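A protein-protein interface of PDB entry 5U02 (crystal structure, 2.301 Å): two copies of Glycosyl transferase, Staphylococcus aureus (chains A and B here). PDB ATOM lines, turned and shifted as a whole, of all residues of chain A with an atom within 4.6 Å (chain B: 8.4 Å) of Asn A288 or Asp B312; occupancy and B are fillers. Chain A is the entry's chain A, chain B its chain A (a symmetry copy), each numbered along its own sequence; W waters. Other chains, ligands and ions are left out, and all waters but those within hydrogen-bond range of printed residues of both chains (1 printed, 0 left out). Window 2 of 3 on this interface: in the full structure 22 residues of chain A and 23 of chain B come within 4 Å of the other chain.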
ATOM      1  N   LYS A 285      17.750  20.666 -10.825  1.00  0.00           N
ATOM      2  CA  LYS A 285      17.213  19.314 -10.884  1.00  0.00           C
ATOM      3  C   LYS A 285      15.792  19.399 -11.424  1.00  0.00           C
ATOM      4  O   LYS A 285      14.948  20.094 -10.848  1.00  0.00           O
ATOM      5  CB  LYS A 285      17.245  18.653  -9.505  1.00  0.00           C
ATOM      6  CG  LYS A 285      16.578  17.288  -9.428  1.00  0.00           C
ATOM      7  CD  LYS A 285      16.767  16.687  -8.040  1.00  0.00           C
ATOM      8  CE  LYS A 285      15.910  15.449  -7.834  1.00  0.00           C
ATOM      9  NZ  LYS A 285      16.195  14.802  -6.523  1.00  0.00           N
ATOM     10  N   GLY A 286      15.531  18.700 -12.527  1.00  0.00           N
ATOM     11  CA  GLY A 286      14.270  18.899 -13.219  1.00  0.00           C
ATOM     12  C   GLY A 286      14.225  20.296 -13.808  1.00  0.00           C
ATOM     13  O   GLY A 286      15.221  20.808 -14.330  1.00  0.00           O
ATOM     14  N   LYS A 287      13.059  20.935 -13.709  1.00  0.00           N
ATOM     15  CA  LYS A 287      12.911  22.315 -14.145  1.00  0.00           C
ATOM     16  C   LYS A 287      12.534  23.276 -13.029  1.00  0.00           C
ATOM     17  O   LYS A 287      12.502  24.488 -13.269  1.00  0.00           O
ATOM     18  CB  LYS A 287      11.861  22.418 -15.263  1.00  0.00           C
ATOM     19  CG  LYS A 287      12.206  21.606 -16.500  1.00  0.00           C
ATOM     20  CD  LYS A 287      13.586  21.977 -17.043  1.00  0.00           C
ATOM     21  CE  LYS A 287      13.632  23.422 -17.532  1.00  0.00           C
ATOM     22  NZ  LYS A 287      14.969  24.046 -17.319  1.00  0.00           N
ATOM     23  N   ASN A 288      12.272  22.783 -11.815  1.00  0.00           N
ATOM     24  CA  ASN A 288      11.745  23.639 -10.760  1.00  0.00           C
ATOM     25  C   ASN A 288      12.440  23.419  -9.419  1.00  0.00           C
ATOM     26  O   ASN A 288      11.911  23.841  -8.384  1.00  0.00           O
ATOM     27  CB  ASN A 288      10.230  23.419 -10.605  1.00  0.00           C
ATOM     28  CG  ASN A 288       9.878  21.988 -10.202  1.00  0.00           C
ATOM     29  OD1 ASN A 288      10.696  21.071 -10.324  1.00  0.00           O
ATOM     30  ND2 ASN A 288       8.653  21.793  -9.730  1.00  0.00           N
ATOM     31  N   LYS A 289      13.607  22.777  -9.399  1.00  0.00           N
ATOM     32  CA  LYS A 289      14.285  22.453  -8.149  1.00  0.00           C
ATOM     33  C   LYS A 289      15.745  22.872  -8.219  1.00  0.00           C
ATOM     34  O   LYS A 289      16.462  22.506  -9.159  1.00  0.00           O
ATOM     35  CB  LYS A 289      14.179  20.958  -7.828  1.00  0.00           C
ATOM     36  CG  LYS A 289      12.800  20.532  -7.336  1.00  0.00           C
ATOM     37  CD  LYS A 289      12.684  19.014  -7.208  1.00  0.00           C
ATOM     38  CE  LYS A 289      11.306  18.621  -6.695  1.00  0.00           C
ATOM     39  NZ  LYS A 289      11.031  17.162  -6.825  1.00  0.00           N
ATOM     40  N   ILE A 290      16.178  23.634  -7.220  1.00  0.00           N
ATOM     41  CA  ILE A 290      17.569  24.040  -7.068  1.00  0.00           C
ATOM     42  C   ILE A 290      18.161  23.229  -5.923  1.00  0.00           C
ATOM     43  O   ILE A 290      17.555  23.126  -4.848  1.00  0.00           O
ATOM     44  CB  ILE A 290      17.680  25.552  -6.819  1.00  0.00           C
ATOM     45  CG1 ILE A 290      17.037  26.311  -7.984  1.00  0.00           C
ATOM     46  CG2 ILE A 290      19.138  25.972  -6.650  1.00  0.00           C
ATOM     47  CD1 ILE A 290      16.857  27.795  -7.743  1.00  0.00           C
ATOM     48  N   ILE A 329      15.405  23.456  -3.033  1.00  0.00           N
ATOM     49  CA  ILE A 329      14.548  24.628  -3.101  1.00  0.00           C
ATOM     50  C   ILE A 329      13.538  24.347  -4.201  1.00  0.00           C
ATOM     51  O   ILE A 329      13.872  24.394  -5.390  1.00  0.00           O
ATOM     52  CB  ILE A 329      15.338  25.913  -3.366  1.00  0.00           C
ATOM     53  CG1 ILE A 329      16.316  26.173  -2.213  1.00  0.00           C
ATOM     54  CG2 ILE A 329      14.386  27.092  -3.531  1.00  0.00           C
ATOM     55  CD1 ILE A 329      17.217  27.373  -2.417  1.00  0.00           C
ATOM     56  N   LEU A 330      12.309  24.020  -3.801  1.00  0.00           N
ATOM     57  CA  LEU A 330      11.222  23.724  -4.735  1.00  0.00           C
ATOM     58  C   LEU A 330      10.605  25.042  -5.185  1.00  0.00           C
ATOM     59  O   LEU A 330       9.851  25.673  -4.442  1.00  0.00           O
ATOM     60  CB  LEU A 330      10.185  22.821  -4.079  1.00  0.00           C
ATOM     61  CG  LEU A 330       8.942  22.476  -4.899  1.00  0.00           C
ATOM     62  CD1 LEU A 330       9.330  21.741  -6.176  1.00  0.00           C
ATOM     63  CD2 LEU A 330       7.951  21.654  -4.078  1.00  0.00           C
ATOM     64  N   LEU A 331      10.921  25.457  -6.411  1.00  0.00           N
ATOM     65  CA  LEU A 331      10.489  26.750  -6.919  1.00  0.00           C
ATOM     66  C   LEU A 331       9.002  26.739  -7.261  1.00  0.00           C
ATOM     67  O   LEU A 331       8.394  25.690  -7.492  1.00  0.00           O
ATOM     68  CB  LEU A 331      11.297  27.133  -8.158  1.00  0.00           C
ATOM     69  CG  LEU A 331      12.795  27.326  -7.956  1.00  0.00           C
ATOM     70  CD1 LEU A 331      13.467  27.558  -9.291  1.00  0.00           C
ATOM     71  CD2 LEU A 331      13.037  28.497  -7.020  1.00  0.00           C
ATOM     72  N   LYS A 333       7.731  28.015  -9.955  1.00  0.00           N
ATOM     73  CA  LYS A 333       7.556  27.865 -11.392  1.00  0.00           C
ATOM     74  C   LYS A 333       8.843  27.305 -11.980  1.00  0.00           C
ATOM     75  O   LYS A 333       9.853  27.152 -11.289  1.00  0.00           O
ATOM     76  CB  LYS A 333       7.188  29.197 -12.055  1.00  0.00           C
ATOM     77  CG  LYS A 333       8.317  30.213 -12.058  1.00  0.00           C
ATOM     78  CD  LYS A 333       7.980  31.409 -12.934  1.00  0.00           C
ATOM     79  CE  LYS A 333       9.184  32.320 -13.093  1.00  0.00           C
ATOM     80  NZ  LYS A 333       8.916  33.455 -14.025  1.00  0.00           N
ATOM     81  N   ASP A 334       8.797  26.998 -13.272  1.00  0.00           N
ATOM     82  CA  ASP A 334       9.980  26.502 -13.960  1.00  0.00           C
ATOM     83  C   ASP A 334      10.991  27.624 -14.171  1.00  0.00           C
ATOM     84  O   ASP A 334      10.633  28.796 -14.322  1.00  0.00           O
ATOM     85  CB  ASP A 334       9.603  25.891 -15.311  1.00  0.00           C
ATOM     86  CG  ASP A 334       8.983  24.516 -15.181  1.00  0.00           C
ATOM     87  OD1 ASP A 334       9.034  23.936 -14.078  1.00  0.00           O
ATOM     88  OD2 ASP A 334       8.450  24.009 -16.191  1.00  0.00           O
ATOM     89  N   VAL B 309       2.267  23.386  -0.195  1.00  0.00           N
ATOM     90  CA  VAL B 309       3.296  22.603  -0.861  1.00  0.00           C
ATOM     91  C   VAL B 309       2.657  21.322  -1.370  1.00  0.00           C
ATOM     92  O   VAL B 309       1.990  20.606  -0.612  1.00  0.00           O
ATOM     93  CB  VAL B 309       4.472  22.290   0.080  1.00  0.00           C
ATOM     94  CG1 VAL B 309       5.477  21.384  -0.615  1.00  0.00           C
ATOM     95  CG2 VAL B 309       5.134  23.569   0.546  1.00  0.00           C
ATOM     96  N   LEU B 310       2.838  21.052  -2.658  1.00  0.00           N
ATOM     97  CA  LEU B 310       2.513  19.762  -3.242  1.00  0.00           C
ATOM     98  C   LEU B 310       3.802  18.979  -3.456  1.00  0.00           C
ATOM     99  O   LEU B 310       4.905  19.480  -3.235  1.00  0.00           O
ATOM    100  CB  LEU B 310       1.742  19.936  -4.556  1.00  0.00           C
ATOM    101  CG  LEU B 310       0.393  20.655  -4.438  1.00  0.00           C
ATOM    102  CD1 LEU B 310       0.528  22.135  -4.756  1.00  0.00           C
ATOM    103  CD2 LEU B 310      -0.663  20.004  -5.320  1.00  0.00           C
ATOM    104  N   LYS B 311       3.652  17.728  -3.891  1.00  0.00           N
ATOM    105  CA  LYS B 311       4.809  16.845  -3.983  1.00  0.00           C
ATOM    106  C   LYS B 311       5.787  17.280  -5.069  1.00  0.00           C
ATOM    107  O   LYS B 311       6.972  16.935  -4.996  1.00  0.00           O
ATOM    108  CB  LYS B 311       4.343  15.405  -4.211  1.00  0.00           C
ATOM    109  CG  LYS B 311       5.448  14.365  -4.184  1.00  0.00           C
ATOM    110  CD  LYS B 311       5.614  13.712  -5.540  1.00  0.00           C
ATOM    111  CE  LYS B 311       6.624  12.580  -5.481  1.00  0.00           C
ATOM    112  NZ  LYS B 311       8.009  13.076  -5.692  1.00  0.00           N
ATOM    113  N   ASP B 312       5.332  18.051  -6.057  1.00  0.00           N
ATOM    114  CA  ASP B 312       6.248  18.574  -7.061  1.00  0.00           C
ATOM    115  C   ASP B 312       5.908  20.013  -7.441  1.00  0.00           C
ATOM    116  O   ASP B 312       6.213  20.448  -8.557  1.00  0.00           O
ATOM    117  CB  ASP B 312       6.259  17.685  -8.307  1.00  0.00           C
ATOM    118  CG  ASP B 312       7.581  17.748  -9.057  1.00  0.00           C
ATOM    119  OD1 ASP B 312       8.640  17.795  -8.391  1.00  0.00           O
ATOM    120  OD2 ASP B 312       7.565  17.744 -10.308  1.00  0.00           O
ATOM    121  N   ASP B 313       5.295  20.770  -6.534  1.00  0.00           N
ATOM    122  CA  ASP B 313       4.919  22.146  -6.833  1.00  0.00           C
ATOM    123  C   ASP B 313       4.632  22.869  -5.524  1.00  0.00           C
ATOM    124  O   ASP B 313       4.385  22.239  -4.491  1.00  0.00           O
ATOM    125  CB  ASP B 313       3.705  22.198  -7.768  1.00  0.00           C
ATOM    126  CG  ASP B 313       3.475  23.570  -8.359  1.00  0.00           C
ATOM    127  OD1 ASP B 313       4.441  24.350  -8.464  1.00  0.00           O
ATOM    128  OD2 ASP B 313       2.321  23.864  -8.728  1.00  0.00           O
ATOM    129  N   MET B 314       4.679  24.200  -5.573  1.00  0.00           N
ATOM    130  CA  MET B 314       4.353  25.007  -4.405  1.00  0.00           C
ATOM    131  C   MET B 314       3.660  26.285  -4.858  1.00  0.00           C
ATOM    132  O   MET B 314       3.881  26.765  -5.973  1.00  0.00           O
ATOM    133  CB  MET B 314       5.608  25.297  -3.548  1.00  0.00           C
ATOM    134  CG  MET B 314       6.643  26.312  -4.072  1.00  0.00           C
ATOM    135  SD  MET B 314       6.213  28.048  -3.855  1.00  0.00           S
ATOM    136  CE  MET B 314       6.144  28.157  -2.077  1.00  0.00           C
ATOM    137  N   ILE B 315       2.789  26.810  -3.999  1.00  0.00           N
ATOM    138  CA  ILE B 315       2.021  28.016  -4.284  1.00  0.00           C
ATOM    139  C   ILE B 315       2.038  28.905  -3.048  1.00  0.00           C
ATOM    140  O   ILE B 315       1.715  28.449  -1.945  1.00  0.00           O
ATOM    141  CB  ILE B 315       0.564  27.708  -4.686  1.00  0.00           C
ATOM    142  CG1 ILE B 315       0.496  26.574  -5.709  1.00  0.00           C
ATOM    143  CG2 ILE B 315      -0.106  28.959  -5.252  1.00  0.00           C
ATOM    144  CD1 ILE B 315      -0.917  26.139  -6.024  1.00  0.00           C
ATOM    145  N   LYS B 333      -2.008  31.973  -7.459  1.00  0.00           N
ATOM    146  CA  LYS B 333      -2.500  31.484  -8.738  1.00  0.00           C
ATOM    147  C   LYS B 333      -3.635  30.503  -8.476  1.00  0.00           C
ATOM    148  O   LYS B 333      -3.933  30.155  -7.330  1.00  0.00           O
ATOM    149  CB  LYS B 333      -1.385  30.820  -9.553  1.00  0.00           C
ATOM    150  CG  LYS B 333      -0.896  29.507  -8.968  1.00  0.00           C
ATOM    151  CD  LYS B 333       0.026  28.781  -9.936  1.00  0.00           C
ATOM    152  CE  LYS B 333       0.349  27.386  -9.432  1.00  0.00           C
ATOM    153  NZ  LYS B 333       1.175  26.611 -10.404  1.00  0.00           N
ATOM    154  N   ASP B 339      -5.579  18.784  -7.723  1.00  0.00           N
ATOM    155  CA  ASP B 339      -4.312  18.984  -7.026  1.00  0.00           C
ATOM    156  C   ASP B 339      -4.513  19.492  -5.607  1.00  0.00           C
ATOM    157  O   ASP B 339      -3.680  19.220  -4.734  1.00  0.00           O
ATOM    158  CB  ASP B 339      -3.420  19.951  -7.803  1.00  0.00           C
ATOM    159  CG  ASP B 339      -2.946  19.377  -9.119  1.00  0.00           C
ATOM    160  OD1 ASP B 339      -1.953  19.892  -9.670  1.00  0.00           O
ATOM    161  OD2 ASP B 339      -3.553  18.398  -9.597  1.00  0.00           O
ATOM    162  N   ASN B 342      -4.120  16.975  -3.129  1.00  0.00           N
ATOM    163  CA  ASN B 342      -2.770  16.452  -2.954  1.00  0.00           C
ATOM    164  C   ASN B 342      -1.852  17.430  -2.228  1.00  0.00           C
ATOM    165  O   ASN B 342      -0.630  17.365  -2.393  1.00  0.00           O
ATOM    166  CB  ASN B 342      -2.169  16.078  -4.308  1.00  0.00           C
ATOM    167  CG  ASN B 342      -2.457  14.642  -4.699  1.00  0.00           C
ATOM    168  OD1 ASN B 342      -1.599  13.766  -4.566  1.00  0.00           O
ATOM    169  ND2 ASN B 342      -3.664  14.392  -5.189  1.00  0.00           N
ATOM    170  N   VAL B 344       0.437  18.409   0.459  1.00  0.00           N
ATOM    171  CA  VAL B 344       1.201  17.650   1.436  1.00  0.00           C
ATOM    172  C   VAL B 344       1.531  18.496   2.663  1.00  0.00           C
ATOM    173  O   VAL B 344       1.628  17.964   3.774  1.00  0.00           O
ATOM    174  CB  VAL B 344       2.474  17.096   0.767  1.00  0.00           C
ATOM    175  CG1 VAL B 344       3.544  16.752   1.790  1.00  0.00           C
ATOM    176  CG2 VAL B 344       2.137  15.873  -0.077  1.00  0.00           C
HETATM  177  O   HOH W   1       5.361  21.538 -10.818  1.00  0.00           O
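Water W1 bridges O of Asp B312 (2.7 Å) and ND2 of Asn A288 (3.5 Å).
Of the 11 printed residues of chain A, 4 touch a printed residue of chain B. Hydrophobic or aromatic side chains of chain A within 4 Å of the printed part of chain B: Leu A330. Along chain A the printed residues that touch a printed residue of chain B span positions 288 to 331. Printed residues of chain B that touch a printed residue of chain A: Leu B310, Asp B312, Asp B313 and Met B314. Hydrophobic or aromatic side chains of chain B that line the printed part of chain A: Met B314.
Position printed for both chains: 333.
The backbone carbonyl oxygen (O) of Asp B312 sits at hydrogen-bond distance from the side-chain amide nitrogen (ND2) of Asn A288 (3.0 Å). The side-chain carboxylate (OD1) of Asp B312 is in salt-bridge range of the side-chain amino group (NZ) of Lys A289 (2.9 Å).
N of Leu A331 sits at hydrogen-bond distance from O of Asn A288 (2.7 Å). NZ of Lys B333 is in salt-bridge range of OD2 of Asp B313.
Of chain B, only Asp B312 comes within 4 Å of Asn A288. Lys A289 touches just one residue of chain B: Asp B312. Of the printed residues of chain B, Leu A330 touches Leu B310, Asp B313 and Met B314. Of the printed residues of chain B, Leu A331 touches Met B314. Asp B312 touches two residues of chain A. Of the printed residues of chain A, Asp B313 touches Leu A330. The nearest residue of chain B that does not touch Asn A288 is Asp B313 (4.7 Å). The nearest residue of chain A that does not touch Asp B312 is Leu A330 (4.04 Å). The nearest printed residue of chain A that does not touch Met B314 is Lys A333 (5.7 Å).
Leu B310 touches Leu A330 (O to CD2, 3.8 Å). Asp B313 touches Leu A330 (O to CD2, 3.6 Å). Met B314 touches Leu A330 (CG to O, 3.3 Å). Leu A331 touches Met B314 (O to CG, 3.9 Å).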
